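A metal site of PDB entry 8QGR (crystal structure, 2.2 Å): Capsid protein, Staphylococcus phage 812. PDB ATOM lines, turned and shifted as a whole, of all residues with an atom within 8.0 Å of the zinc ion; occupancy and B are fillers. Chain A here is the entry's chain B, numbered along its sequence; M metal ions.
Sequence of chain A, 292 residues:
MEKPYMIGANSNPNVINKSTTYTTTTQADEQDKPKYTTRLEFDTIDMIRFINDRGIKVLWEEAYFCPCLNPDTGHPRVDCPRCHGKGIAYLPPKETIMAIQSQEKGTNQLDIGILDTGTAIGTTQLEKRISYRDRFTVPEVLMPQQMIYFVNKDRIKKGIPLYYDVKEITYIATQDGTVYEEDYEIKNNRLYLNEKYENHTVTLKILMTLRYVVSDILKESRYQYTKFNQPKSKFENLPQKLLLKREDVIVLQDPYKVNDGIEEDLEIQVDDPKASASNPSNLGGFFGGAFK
Within 4 Å of the zinc ion: Cys 66, Cys 68, Cys 80 and Cys 83. Along chain A the residues within 4 Å of the zinc ion span positions 66 to 83. The nearest printed residue that does not touch the zinc ion is Arg 82 (4.4 Å).
O of Cys 68 sits at hydrogen-bond distance from NE of Arg 77 (2.7 Å). NE of Arg 82 sits close to SG of Cys 66. O of Gly 87 lies within hydrogen-bond range of N of Cys 66. SG of Cys 80 lies close to N of Arg 82. A ring nitrogen (ND1) of His 84 sits close to the backbone carbonyl oxygen (O) of Cys 80 (3.5 Å). The side-chain sulfur of Cys 83 lies close to the backbone NH of Gly 85 (3.4 Å). The side-chain sulfur (SG) of Cys 83 sits close to the backbone NH (N) of Gly 87. N of Lys 86 lies close to SG of Cys 83, 3.7 Å away.
The zinc ion is bound by the side-chain sulfur of Cys 68, the side-chain sulfur of Cys 66, the side-chain sulfur of Cys 80 and the side-chain sulfur of Cys 83. The zinc ion has four donor atoms within binding distance.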
ATOM      1  N   TYR A  64       7.166  -0.094 -26.548  1.00  0.00           N
ATOM      2  CA  TYR A  64       6.923  -1.526 -26.550  1.00  0.00           C
ATOM      3  C   TYR A  64       7.542  -2.133 -25.308  1.00  0.00           C
ATOM      4  O   TYR A  64       8.397  -1.507 -24.671  1.00  0.00           O
ATOM      5  CB  TYR A  64       7.507  -2.188 -27.807  1.00  0.00           C
ATOM      6  CG  TYR A  64       8.988  -2.031 -27.977  1.00  0.00           C
ATOM      7  CD1 TYR A  64       9.548  -0.862 -28.454  1.00  0.00           C
ATOM      8  CD2 TYR A  64       9.847  -3.052 -27.603  1.00  0.00           C
ATOM      9  CE1 TYR A  64      10.915  -0.728 -28.597  1.00  0.00           C
ATOM     10  CE2 TYR A  64      11.213  -2.934 -27.750  1.00  0.00           C
ATOM     11  CZ  TYR A  64      11.754  -1.775 -28.249  1.00  0.00           C
ATOM     12  OH  TYR A  64      13.125  -1.686 -28.360  1.00  0.00           O
ATOM     13  N   PHE A  65       7.109  -3.344 -24.938  1.00  0.00           N
ATOM     14  CA  PHE A  65       7.699  -4.064 -23.821  1.00  0.00           C
ATOM     15  C   PHE A  65       9.084  -4.556 -24.222  1.00  0.00           C
ATOM     16  O   PHE A  65       9.243  -5.194 -25.268  1.00  0.00           O
ATOM     17  CB  PHE A  65       6.812  -5.221 -23.361  1.00  0.00           C
ATOM     18  CG  PHE A  65       5.542  -4.789 -22.683  1.00  0.00           C
ATOM     19  CD1 PHE A  65       5.593  -4.156 -21.449  1.00  0.00           C
ATOM     20  CD2 PHE A  65       4.314  -4.974 -23.278  1.00  0.00           C
ATOM     21  CE1 PHE A  65       4.428  -3.748 -20.825  1.00  0.00           C
ATOM     22  CE2 PHE A  65       3.144  -4.557 -22.658  1.00  0.00           C
ATOM     23  CZ  PHE A  65       3.204  -3.960 -21.429  1.00  0.00           C
ATOM     24  N   CYS A  66      10.073  -4.270 -23.371  1.00  0.00           N
ATOM     25  CA  CYS A  66      11.453  -4.589 -23.670  1.00  0.00           C
ATOM     26  C   CYS A  66      11.674  -6.090 -23.507  1.00  0.00           C
ATOM     27  O   CYS A  66      11.361  -6.650 -22.455  1.00  0.00           O
ATOM     28  CB  CYS A  66      12.431  -3.853 -22.761  1.00  0.00           C
ATOM     29  SG  CYS A  66      14.134  -3.869 -23.383  1.00  0.00           S
ATOM     30  N   PRO A  67      12.217  -6.759 -24.537  1.00  0.00           N
ATOM     31  CA  PRO A  67      12.483  -8.199 -24.468  1.00  0.00           C
ATOM     32  C   PRO A  67      13.779  -8.627 -23.778  1.00  0.00           C
ATOM     33  O   PRO A  67      14.298  -9.700 -24.078  1.00  0.00           O
ATOM     34  CB  PRO A  67      12.562  -8.574 -25.962  1.00  0.00           C
ATOM     35  CG  PRO A  67      13.154  -7.342 -26.627  1.00  0.00           C
ATOM     36  CD  PRO A  67      12.584  -6.175 -25.844  1.00  0.00           C
ATOM     37  N   CYS A  68      14.290  -7.814 -22.837  1.00  0.00           N
ATOM     38  CA  CYS A  68      15.514  -8.155 -22.124  1.00  0.00           C
ATOM     39  C   CYS A  68      15.186  -8.994 -20.897  1.00  0.00           C
ATOM     40  O   CYS A  68      16.091  -9.503 -20.233  1.00  0.00           O
ATOM     41  CB  CYS A  68      16.253  -6.912 -21.641  1.00  0.00           C
ATOM     42  SG  CYS A  68      15.320  -5.932 -20.427  1.00  0.00           S
ATOM     43  N   LEU A  69      13.899  -9.150 -20.603  1.00  0.00           N
ATOM     44  CA  LEU A  69      13.451  -9.816 -19.402  1.00  0.00           C
ATOM     45  C   LEU A  69      14.240 -11.102 -19.152  1.00  0.00           C
ATOM     46  O   LEU A  69      14.529 -11.852 -20.096  1.00  0.00           O
ATOM     47  CB  LEU A  69      11.969 -10.179 -19.545  1.00  0.00           C
ATOM     48  CG  LEU A  69      11.002  -9.023 -19.759  1.00  0.00           C
ATOM     49  CD1 LEU A  69       9.586  -9.502 -19.521  1.00  0.00           C
ATOM     50  CD2 LEU A  69      11.347  -7.832 -18.867  1.00  0.00           C
ATOM     51  N   HIS A  75      11.976 -10.140 -14.563  1.00  0.00           N
ATOM     52  CA  HIS A  75      12.540  -8.810 -14.361  1.00  0.00           C
ATOM     53  C   HIS A  75      13.387  -8.367 -15.535  1.00  0.00           C
ATOM     54  O   HIS A  75      14.160  -9.139 -16.118  1.00  0.00           O
ATOM     55  CB  HIS A  75      13.407  -8.756 -13.102  1.00  0.00           C
ATOM     56  CG  HIS A  75      12.638  -8.746 -11.816  1.00  0.00           C
ATOM     57  ND1 HIS A  75      12.405  -9.881 -11.085  1.00  0.00           N
ATOM     58  CD2 HIS A  75      12.005  -7.753 -11.185  1.00  0.00           C
ATOM     59  CE1 HIS A  75      11.677  -9.576 -10.019  1.00  0.00           C
ATOM     60  NE2 HIS A  75      11.423  -8.283 -10.065  1.00  0.00           N
ATOM     61  N   PRO A  76      13.295  -7.076 -15.921  1.00  0.00           N
ATOM     62  CA  PRO A  76      14.210  -6.508 -16.899  1.00  0.00           C
ATOM     63  C   PRO A  76      15.652  -6.583 -16.429  1.00  0.00           C
ATOM     64  O   PRO A  76      15.915  -6.779 -15.240  1.00  0.00           O
ATOM     65  CB  PRO A  76      13.747  -5.045 -17.025  1.00  0.00           C
ATOM     66  CG  PRO A  76      12.306  -5.067 -16.547  1.00  0.00           C
ATOM     67  CD  PRO A  76      12.272  -6.126 -15.455  1.00  0.00           C
ATOM     68  N   ARG A  77      16.588  -6.439 -17.362  1.00  0.00           N
ATOM     69  CA  ARG A  77      17.990  -6.382 -17.004  1.00  0.00           C
ATOM     70  C   ARG A  77      18.251  -5.002 -16.416  1.00  0.00           C
ATOM     71  O   ARG A  77      17.889  -3.990 -17.002  1.00  0.00           O
ATOM     72  CB  ARG A  77      18.885  -6.619 -18.227  1.00  0.00           C
ATOM     73  CG  ARG A  77      18.560  -7.866 -19.012  1.00  0.00           C
ATOM     74  CD  ARG A  77      18.722  -9.134 -18.183  1.00  0.00           C
ATOM     75  NE  ARG A  77      18.231 -10.310 -18.882  1.00  0.00           N
ATOM     76  CZ  ARG A  77      18.401 -11.553 -18.465  1.00  0.00           C
ATOM     77  NH1 ARG A  77      17.960 -12.572 -19.187  1.00  0.00           N
ATOM     78  NH2 ARG A  77      19.041 -11.789 -17.335  1.00  0.00           N
ATOM     79  N   VAL A  78      18.931  -5.001 -15.269  1.00  0.00           N
ATOM     80  CA  VAL A  78      19.240  -3.809 -14.497  1.00  0.00           C
ATOM     81  C   VAL A  78      19.781  -2.691 -15.381  1.00  0.00           C
ATOM     82  O   VAL A  78      19.365  -1.536 -15.261  1.00  0.00           O
ATOM     83  CB  VAL A  78      20.252  -4.176 -13.399  1.00  0.00           C
ATOM     84  CG1 VAL A  78      20.873  -2.947 -12.759  1.00  0.00           C
ATOM     85  CG2 VAL A  78      19.613  -5.056 -12.341  1.00  0.00           C
ATOM     86  N   ASP A  79      20.767  -3.026 -16.215  1.00  0.00           N
ATOM     87  CA  ASP A  79      21.442  -2.003 -16.992  1.00  0.00           C
ATOM     88  C   ASP A  79      21.150  -2.146 -18.476  1.00  0.00           C
ATOM     89  O   ASP A  79      21.968  -1.770 -19.315  1.00  0.00           O
ATOM     90  CB  ASP A  79      22.935  -1.968 -16.670  1.00  0.00           C
ATOM     91  CG  ASP A  79      23.218  -1.461 -15.258  1.00  0.00           C
ATOM     92  OD1 ASP A  79      22.652  -0.384 -14.882  1.00  0.00           O
ATOM     93  OD2 ASP A  79      23.980  -2.122 -14.539  1.00  0.00           O
ATOM     94  N   CYS A  80      19.942  -2.590 -18.807  1.00  0.00           N
ATOM     95  CA  CYS A  80      19.543  -2.664 -20.202  1.00  0.00           C
ATOM     96  C   CYS A  80      19.594  -1.263 -20.803  1.00  0.00           C
ATOM     97  O   CYS A  80      19.006  -0.331 -20.257  1.00  0.00           O
ATOM     98  CB  CYS A  80      18.146  -3.240 -20.331  1.00  0.00           C
ATOM     99  SG  CYS A  80      17.469  -3.208 -22.006  1.00  0.00           S
ATOM    100  N   PRO A  81      20.295  -1.049 -21.945  1.00  0.00           N
ATOM    101  CA  PRO A  81      20.337   0.265 -22.578  1.00  0.00           C
ATOM    102  C   PRO A  81      19.024   0.705 -23.210  1.00  0.00           C
ATOM    103  O   PRO A  81      18.822   1.904 -23.425  1.00  0.00           O
ATOM    104  CB  PRO A  81      21.430   0.149 -23.649  1.00  0.00           C
ATOM    105  CG  PRO A  81      21.503  -1.337 -23.943  1.00  0.00           C
ATOM    106  CD  PRO A  81      21.121  -2.038 -22.644  1.00  0.00           C
ATOM    107  N   ARG A  82      18.113  -0.230 -23.479  1.00  0.00           N
ATOM    108  CA  ARG A  82      16.835   0.127 -24.088  1.00  0.00           C
ATOM    109  C   ARG A  82      15.838   0.624 -23.049  1.00  0.00           C
ATOM    110  O   ARG A  82      15.163   1.625 -23.281  1.00  0.00           O
ATOM    111  CB  ARG A  82      16.218  -1.048 -24.841  1.00  0.00           C
ATOM    112  CG  ARG A  82      16.982  -1.420 -26.104  1.00  0.00           C
ATOM    113  CD  ARG A  82      16.264  -2.477 -26.932  1.00  0.00           C
ATOM    114  NE  ARG A  82      15.968  -3.622 -26.089  1.00  0.00           N
ATOM    115  CZ  ARG A  82      16.620  -4.768 -26.134  1.00  0.00           C
ATOM    116  NH1 ARG A  82      16.328  -5.736 -25.278  1.00  0.00           N
ATOM    117  NH2 ARG A  82      17.589  -4.949 -27.018  1.00  0.00           N
ATOM    118  N   CYS A  83      15.732  -0.081 -21.916  1.00  0.00           N
ATOM    119  CA  CYS A  83      14.701   0.254 -20.948  1.00  0.00           C
ATOM    120  C   CYS A  83      15.285   0.652 -19.595  1.00  0.00           C
ATOM    121  O   CYS A  83      14.515   0.990 -18.699  1.00  0.00           O
ATOM    122  CB  CYS A  83      13.730  -0.898 -20.733  1.00  0.00           C
ATOM    123  SG  CYS A  83      14.468  -2.315 -19.857  1.00  0.00           S
ATOM    124  N   HIS A  84      16.608   0.541 -19.428  1.00  0.00           N
ATOM    125  CA  HIS A  84      17.285   0.935 -18.196  1.00  0.00           C
ATOM    126  C   HIS A  84      16.756   0.147 -16.995  1.00  0.00           C
ATOM    127  O   HIS A  84      16.816   0.621 -15.869  1.00  0.00           O
ATOM    128  CB  HIS A  84      17.116   2.449 -17.961  1.00  0.00           C
ATOM    129  CG  HIS A  84      17.507   3.237 -19.161  1.00  0.00           C
ATOM    130  ND1 HIS A  84      18.741   3.097 -19.764  1.00  0.00           N
ATOM    131  CD2 HIS A  84      16.818   4.097 -19.916  1.00  0.00           C
ATOM    132  CE1 HIS A  84      18.790   3.883 -20.834  1.00  0.00           C
ATOM    133  NE2 HIS A  84      17.635   4.493 -20.943  1.00  0.00           N
ATOM    134  N   GLY A  85      16.249  -1.058 -17.238  1.00  0.00           N
ATOM    135  CA  GLY A  85      15.724  -1.875 -16.158  1.00  0.00           C
ATOM    136  C   GLY A  85      14.224  -1.689 -15.886  1.00  0.00           C
ATOM    137  O   GLY A  85      13.696  -2.359 -14.994  1.00  0.00           O
ATOM    138  N   LYS A  86      13.521  -0.827 -16.623  1.00  0.00           N
ATOM    139  CA  LYS A  86      12.115  -0.563 -16.306  1.00  0.00           C
ATOM    140  C   LYS A  86      11.163  -1.407 -17.161  1.00  0.00           C
ATOM    141  O   LYS A  86       9.972  -1.468 -16.840  1.00  0.00           O
ATOM    142  CB  LYS A  86      11.750   0.909 -16.491  1.00  0.00           C
ATOM    143  CG  LYS A  86      12.546   1.887 -15.631  1.00  0.00           C
ATOM    144  CD  LYS A  86      12.594   1.524 -14.164  1.00  0.00           C
ATOM    145  CE  LYS A  86      13.089   2.692 -13.326  1.00  0.00           C
ATOM    146  NZ  LYS A  86      13.224   2.316 -11.899  1.00  0.00           N
ATOM    147  N   GLY A  87      11.651  -2.020 -18.240  1.00  0.00           N
ATOM    148  CA  GLY A  87      10.883  -3.049 -18.947  1.00  0.00           C
ATOM    149  C   GLY A  87      10.025  -2.504 -20.086  1.00  0.00           C
ATOM    150  O   GLY A  87       9.331  -3.276 -20.776  1.00  0.00           O
ATOM    151  N   ILE A  88      10.079  -1.188 -20.280  1.00  0.00           N
ATOM    152  CA  ILE A  88       9.436  -0.537 -21.402  1.00  0.00           C
ATOM    153  C   ILE A  88      10.490   0.257 -22.166  1.00  0.00           C
ATOM    154  O   ILE A  88      11.266   0.983 -21.570  1.00  0.00           O
ATOM    155  CB  ILE A  88       8.268   0.346 -20.930  1.00  0.00           C
ATOM    156  CG1 ILE A  88       7.194  -0.515 -20.242  1.00  0.00           C
ATOM    157  CG2 ILE A  88       7.712   1.148 -22.097  1.00  0.00           C
ATOM    158  CD1 ILE A  88       5.966   0.248 -19.810  1.00  0.00           C
ATOM    159  N   ALA A  89      10.502   0.044 -23.489  1.00  0.00           N
ATOM    160  CA  ALA A  89      11.457   0.665 -24.392  1.00  0.00           C
ATOM    161  C   ALA A  89      10.686   1.464 -25.442  1.00  0.00           C
ATOM    162  O   ALA A  89       9.498   1.251 -25.635  1.00  0.00           O
ATOM    163  CB  ALA A  89      12.315  -0.382 -25.046  1.00  0.00           C
HETATM  164 ZN    ZN M   1      15.304  -3.861 -21.405  1.00  0.00          ZN
